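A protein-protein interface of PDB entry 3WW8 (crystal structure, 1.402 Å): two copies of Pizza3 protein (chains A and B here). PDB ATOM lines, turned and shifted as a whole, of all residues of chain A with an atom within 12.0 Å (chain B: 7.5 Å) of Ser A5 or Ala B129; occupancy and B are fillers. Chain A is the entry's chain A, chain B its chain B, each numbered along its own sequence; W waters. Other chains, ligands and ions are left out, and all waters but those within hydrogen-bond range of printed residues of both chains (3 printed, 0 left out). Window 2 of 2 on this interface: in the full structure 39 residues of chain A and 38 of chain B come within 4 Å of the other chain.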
ATOM      1  N   SER A   5      26.040   9.809  16.489  1.00  0.00           N
ATOM      2  CA  SER A   5      27.400   9.383  16.171  1.00  0.00           C
ATOM      3  C   SER A   5      28.356   9.675  17.322  1.00  0.00           C
ATOM      4  O   SER A   5      28.183  10.655  18.049  1.00  0.00           O
ATOM      5  CB  SER A   5      27.902  10.082  14.907  1.00  0.00           C
ATOM      6  OG  SER A   5      29.236   9.696  14.612  1.00  0.00           O
ATOM      7  N   ASN A   6      29.369   8.827  17.479  1.00  0.00           N
ATOM      8  CA  ASN A   6      30.382   9.042  18.501  1.00  0.00           C
ATOM      9  C   ASN A   6      31.732   9.442  17.920  1.00  0.00           C
ATOM     10  O   ASN A   6      32.713   9.562  18.653  1.00  0.00           O
ATOM     11  CB  ASN A   6      30.537   7.796  19.377  1.00  0.00           C
ATOM     12  CG  ASN A   6      29.290   7.494  20.174  1.00  0.00           C
ATOM     13  OD1 ASN A   6      28.603   8.404  20.645  1.00  0.00           O
ATOM     14  ND2 ASN A   6      28.980   6.213  20.322  1.00  0.00           N
ATOM     15  N   THR A   7      31.786   9.646  16.607  1.00  0.00           N
ATOM     16  CA  THR A   7      33.054  10.003  15.970  1.00  0.00           C
ATOM     17  C   THR A   7      32.914  11.204  15.038  1.00  0.00           C
ATOM     18  O   THR A   7      32.231  11.147  14.011  1.00  0.00           O
ATOM     19  CB  THR A   7      33.696   8.827  15.216  1.00  0.00           C
ATOM     20  OG1 THR A   7      33.759   7.687  16.081  1.00  0.00           O
ATOM     21  CG2 THR A   7      35.100   9.193  14.794  1.00  0.00           C
ATOM     22  N   GLN A   8      33.592  12.281  15.414  1.00  0.00           N
ATOM     23  CA  GLN A   8      33.540  13.529  14.672  1.00  0.00           C
ATOM     24  C   GLN A   8      34.241  13.419  13.325  1.00  0.00           C
ATOM     25  O   GLN A   8      35.057  12.512  13.100  1.00  0.00           O
ATOM     26  CB  GLN A   8      34.211  14.636  15.489  1.00  0.00           C
ATOM     27  CG  GLN A   8      35.729  14.510  15.548  1.00  0.00           C
ATOM     28  CD  GLN A   8      36.348  15.367  16.631  1.00  0.00           C
ATOM     29  OE1 GLN A   8      35.655  15.845  17.532  1.00  0.00           O
ATOM     30  NE2 GLN A   8      37.656  15.576  16.551  1.00  0.00           N
ATOM     31  N   THR A   9      33.917  14.349  12.436  1.00  0.00           N
ATOM     32  CA  THR A   9      34.670  14.513  11.205  1.00  0.00           C
ATOM     33  C   THR A   9      35.223  15.929  11.183  1.00  0.00           C
ATOM     34  O   THR A   9      34.693  16.825  11.852  1.00  0.00           O
ATOM     35  CB  THR A   9      33.804  14.238   9.956  1.00  0.00           C
ATOM     36  OG1 THR A   9      32.689  15.139   9.919  1.00  0.00           O
ATOM     37  CG2 THR A   9      33.287  12.811   9.971  1.00  0.00           C
ATOM     38  N   VAL A  10      36.303  16.123  10.441  1.00  0.00           N
ATOM     39  CA  VAL A  10      36.891  17.438  10.281  1.00  0.00           C
ATOM     40  C   VAL A  10      36.476  17.971   8.923  1.00  0.00           C
ATOM     41  O   VAL A  10      36.644  17.301   7.907  1.00  0.00           O
ATOM     42  CB  VAL A  10      38.422  17.366  10.368  1.00  0.00           C
ATOM     43  CG1 VAL A  10      39.038  18.742  10.206  1.00  0.00           C
ATOM     44  CG2 VAL A  10      38.851  16.727  11.689  1.00  0.00           C
ATOM     45  N   TYR B  73      22.955  23.717  23.393  1.00  0.00           N
ATOM     46  CA  TYR B  73      24.316  23.216  23.178  1.00  0.00           C
ATOM     47  C   TYR B  73      25.295  24.307  23.560  1.00  0.00           C
ATOM     48  O   TYR B  73      25.153  25.444  23.128  1.00  0.00           O
ATOM     49  CB  TYR B  73      24.540  22.868  21.706  1.00  0.00           C
ATOM     50  CG  TYR B  73      23.576  21.861  21.141  1.00  0.00           C
ATOM     51  CD1 TYR B  73      22.283  22.224  20.809  1.00  0.00           C
ATOM     52  CD2 TYR B  73      23.963  20.534  20.943  1.00  0.00           C
ATOM     53  CE1 TYR B  73      21.395  21.309  20.295  1.00  0.00           C
ATOM     54  CE2 TYR B  73      23.082  19.602  20.421  1.00  0.00           C
ATOM     55  CZ  TYR B  73      21.801  19.992  20.098  1.00  0.00           C
ATOM     56  OH  TYR B  73      20.926  19.066  19.584  1.00  0.00           O
ATOM     57  N   LYS B  84      25.353  19.410  26.171  1.00  0.00           N
ATOM     58  CA  LYS B  84      23.994  19.762  25.797  1.00  0.00           C
ATOM     59  C   LYS B  84      22.996  19.401  26.884  1.00  0.00           C
ATOM     60  O   LYS B  84      23.237  18.509  27.716  1.00  0.00           O
ATOM     61  CB  LYS B  84      23.589  19.112  24.475  1.00  0.00           C
ATOM     62  CG  LYS B  84      23.412  17.617  24.568  1.00  0.00           C
ATOM     63  CD  LYS B  84      23.016  17.019  23.237  1.00  0.00           C
ATOM     64  CE  LYS B  84      22.849  15.509  23.353  1.00  0.00           C
ATOM     65  NZ  LYS B  84      22.489  14.918  22.035  1.00  0.00           N
ATOM     66  N   LEU B  95      29.093  15.776  24.748  1.00  0.00           N
ATOM     67  CA  LEU B  95      29.150  15.200  23.409  1.00  0.00           C
ATOM     68  C   LEU B  95      30.514  14.562  23.186  1.00  0.00           C
ATOM     69  O   LEU B  95      31.524  15.058  23.684  1.00  0.00           O
ATOM     70  CB  LEU B  95      28.844  16.253  22.340  1.00  0.00           C
ATOM     71  CG  LEU B  95      27.374  16.674  22.278  1.00  0.00           C
ATOM     72  CD1 LEU B  95      27.195  17.759  21.254  1.00  0.00           C
ATOM     73  CD2 LEU B  95      26.473  15.501  21.960  1.00  0.00           C
ATOM     74  N   PRO B  96      30.554  13.455  22.426  1.00  0.00           N
ATOM     75  CA  PRO B  96      31.802  12.699  22.269  1.00  0.00           C
ATOM     76  C   PRO B  96      32.740  13.271  21.201  1.00  0.00           C
ATOM     77  O   PRO B  96      33.231  12.537  20.345  1.00  0.00           O
ATOM     78  CB  PRO B  96      31.309  11.305  21.874  1.00  0.00           C
ATOM     79  CG  PRO B  96      30.050  11.575  21.117  1.00  0.00           C
ATOM     80  CD  PRO B  96      29.406  12.750  21.827  1.00  0.00           C
ATOM     81  N   PHE B  97      32.986  14.579  21.253  1.00  0.00           N
ATOM     82  CA  PHE B  97      34.032  15.178  20.433  1.00  0.00           C
ATOM     83  C   PHE B  97      35.393  14.715  20.946  1.00  0.00           C
ATOM     84  O   PHE B  97      35.511  14.258  22.082  1.00  0.00           O
ATOM     85  CB  PHE B  97      33.960  16.707  20.470  1.00  0.00           C
ATOM     86  CG  PHE B  97      32.831  17.279  19.665  1.00  0.00           C
ATOM     87  CD1 PHE B  97      32.920  17.362  18.282  1.00  0.00           C
ATOM     88  CD2 PHE B  97      31.698  17.768  20.288  1.00  0.00           C
ATOM     89  CE1 PHE B  97      31.890  17.886  17.531  1.00  0.00           C
ATOM     90  CE2 PHE B  97      30.659  18.308  19.538  1.00  0.00           C
ATOM     91  CZ  PHE B  97      30.757  18.368  18.164  1.00  0.00           C
ATOM     92  N   ASP B 109      22.387  21.878  12.878  1.00  0.00           N
ATOM     93  CA  ASP B 109      21.506  21.940  11.706  1.00  0.00           C
ATOM     94  C   ASP B 109      20.176  21.221  11.951  1.00  0.00           C
ATOM     95  O   ASP B 109      19.934  20.705  13.047  1.00  0.00           O
ATOM     96  CB  ASP B 109      22.200  21.454  10.416  1.00  0.00           C
ATOM     97  CG  ASP B 109      22.542  19.976  10.435  1.00  0.00           C
ATOM     98  OD1 ASP B 109      21.961  19.197  11.231  1.00  0.00           O
ATOM     99  OD2 ASP B 109      23.404  19.584   9.619  1.00  0.00           O
ATOM    100  N   ALA B 111      19.097  18.482  10.947  1.00  0.00           N
ATOM    101  CA  ALA B 111      19.261  17.054  11.181  1.00  0.00           C
ATOM    102  C   ALA B 111      19.854  16.750  12.553  1.00  0.00           C
ATOM    103  O   ALA B 111      20.033  15.588  12.907  1.00  0.00           O
ATOM    104  CB  ALA B 111      20.119  16.431  10.086  1.00  0.00           C
ATOM    105  N   GLY B 112      20.161  17.789  13.324  1.00  0.00           N
ATOM    106  CA  GLY B 112      20.758  17.602  14.634  1.00  0.00           C
ATOM    107  C   GLY B 112      22.266  17.425  14.626  1.00  0.00           C
ATOM    108  O   GLY B 112      22.869  17.113  15.656  1.00  0.00           O
ATOM    109  N   THR B 113      22.894  17.603  13.470  1.00  0.00           N
ATOM    110  CA  THR B 113      24.346  17.567  13.417  1.00  0.00           C
ATOM    111  C   THR B 113      24.942  18.799  14.085  1.00  0.00           C
ATOM    112  O   THR B 113      24.474  19.919  13.870  1.00  0.00           O
ATOM    113  CB  THR B 113      24.849  17.465  11.977  1.00  0.00           C
ATOM    114  OG1 THR B 113      24.384  16.232  11.420  1.00  0.00           O
ATOM    115  CG2 THR B 113      26.368  17.474  11.939  1.00  0.00           C
ATOM    116  N   VAL B 114      25.953  18.574  14.923  1.00  0.00           N
ATOM    117  CA  VAL B 114      26.581  19.627  15.713  1.00  0.00           C
ATOM    118  C   VAL B 114      27.935  20.009  15.119  1.00  0.00           C
ATOM    119  O   VAL B 114      28.767  19.150  14.838  1.00  0.00           O
ATOM    120  CB  VAL B 114      26.748  19.193  17.194  1.00  0.00           C
ATOM    121  CG1 VAL B 114      27.392  20.298  18.013  1.00  0.00           C
ATOM    122  CG2 VAL B 114      25.399  18.792  17.791  1.00  0.00           C
ATOM    123  N   LYS B 126      32.609  18.276  13.145  1.00  0.00           N
ATOM    124  CA  LYS B 126      31.195  18.024  12.897  1.00  0.00           C
ATOM    125  C   LYS B 126      30.829  16.669  13.526  1.00  0.00           C
ATOM    126  O   LYS B 126      31.605  15.727  13.448  1.00  0.00           O
ATOM    127  CB  LYS B 126      30.981  18.023  11.375  1.00  0.00           C
ATOM    128  CG  LYS B 126      29.753  17.325  10.839  1.00  0.00           C
ATOM    129  CD  LYS B 126      29.714  17.465   9.325  1.00  0.00           C
ATOM    130  CE  LYS B 126      28.362  17.106   8.726  1.00  0.00           C
ATOM    131  NZ  LYS B 126      28.500  16.853   7.254  1.00  0.00           N
ATOM    132  N   LEU B 127      29.674  16.572  14.173  1.00  0.00           N
ATOM    133  CA  LEU B 127      29.273  15.320  14.815  1.00  0.00           C
ATOM    134  C   LEU B 127      27.783  15.097  14.580  1.00  0.00           C
ATOM    135  O   LEU B 127      26.955  15.848  15.097  1.00  0.00           O
ATOM    136  CB  LEU B 127      29.572  15.386  16.316  1.00  0.00           C
ATOM    137  CG  LEU B 127      29.369  14.143  17.174  1.00  0.00           C
ATOM    138  CD1 LEU B 127      30.372  13.063  16.796  1.00  0.00           C
ATOM    139  CD2 LEU B 127      29.517  14.506  18.638  1.00  0.00           C
ATOM    140  N   ALA B 128      27.444  14.079  13.793  1.00  0.00           N
ATOM    141  CA  ALA B 128      26.043  13.760  13.517  1.00  0.00           C
ATOM    142  C   ALA B 128      25.335  13.257  14.776  1.00  0.00           C
ATOM    143  O   ALA B 128      25.974  12.715  15.677  1.00  0.00           O
ATOM    144  CB  ALA B 128      25.948  12.731  12.409  1.00  0.00           C
ATOM    145  N   ALA B 129      24.018  13.431  14.839  1.00  0.00           N
ATOM    146  CA  ALA B 129      23.250  12.935  15.980  1.00  0.00           C
ATOM    147  C   ALA B 129      23.270  11.410  16.015  1.00  0.00           C
ATOM    148  O   ALA B 129      23.298  10.766  14.964  1.00  0.00           O
ATOM    149  CB  ALA B 129      21.818  13.444  15.921  1.00  0.00           C
HETATM  150  O   HOH W   1      34.812  12.384  18.064  1.00  0.00           O
HETATM  151  O   HOH W   2      29.689  12.344  12.856  1.00  0.00           O
HETATM  152  O   HOH W   3      34.731   9.715  20.510  1.00  0.00           O
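The backbone NH (N) of Thr A7 sits at hydrogen-bond distance from the side-chain hydroxyl (OG) of Ser A5 (3.2 Å).
The backbone carbonyl oxygen (O) of Val B114 lies within hydrogen-bond range of the backbone NH (N) of Leu B127 (2.8 Å).
Water W3 lies within hydrogen-bond range of O of Asn A6 and O of Pro B96.
Water W1 bridges O of Pro B96 and N of Gln A8.
Water W2 lies within hydrogen-bond range of the backbone NH (N) of Ala B128 (3.0 Å), the backbone carbonyl oxygen (O) of Thr A7 (3.0 Å) and the side-chain hydroxyl (OG) of Ser A5 (3.2 Å).
N of Ser A5 lies within hydrogen-bond range of O of Ala B128, 3.0 Å away.
The backbone NH (N) of Ser A5 sits close to the backbone carbonyl oxygen (O) of Ala B129, 3.3 Å away.
The backbone carbonyl oxygen (O) of Thr A9 sits at hydrogen-bond distance from the backbone NH (N) of Lys B126 (2.8 Å).
The backbone carbonyl oxygen (O) of Pro B96 sits close to the backbone carbonyl oxygen (O) of Asn A6 (3.5 Å).
Ser A5 touches just these residues of chain B: Pro B96 (3.7 Å), Leu B127 (3.5 Å), Ala B128 (3.0 Å) and Ala B129 (3.2 Å).
Ala B129 touches just one residue of chain A: Ser A5.
Pro B96 touches just these residues of chain A: Ser A5 and Asn A6.
Thr B113 touches none of the printed residues of chain A.
Leu B127 touches three residues of chain A.
Of the printed residues of chain B, Asn A6 touches Pro B96.
Of the printed residues of chain B, Thr A7 touches Leu B127.
Printed residues of chain A within 4 Å of Phe B97: Gln A8.
Printed residues of chain A within 4 Å of Lys B126: Gln A8 and Thr A9.
Of the printed residues of chain B, Gln A8 touches Phe B97, Lys B126 and Leu B127.
Val B114 touches none of the printed residues of chain A.
The nearest residue of chain A that does not touch Ala B129 is Asn A6 (6.8 Å).
Ser A5 touches Pro B96.
O of Ser A5 touches CD1 of Leu B127, 3.5 Å away.
Thr A7 touches Leu B127 (C to CD1, 3.6 Å).
Gln A8 touches Phe B97.
Lys B126 touches Gln A8 (O to CA, 3.2 Å).
CD1 of Leu B127 touches N of Gln A8 (3.6 Å).
No position is printed for both chains.
Of the 10 pairs that touch across the chains among the printed residues, none has its exchanged pair printed and touching as well.
Of the 14 printed residues of chain B, 6 touch a printed residue of chain A.
Among the printed residues, 10 pairs touch across the chains.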
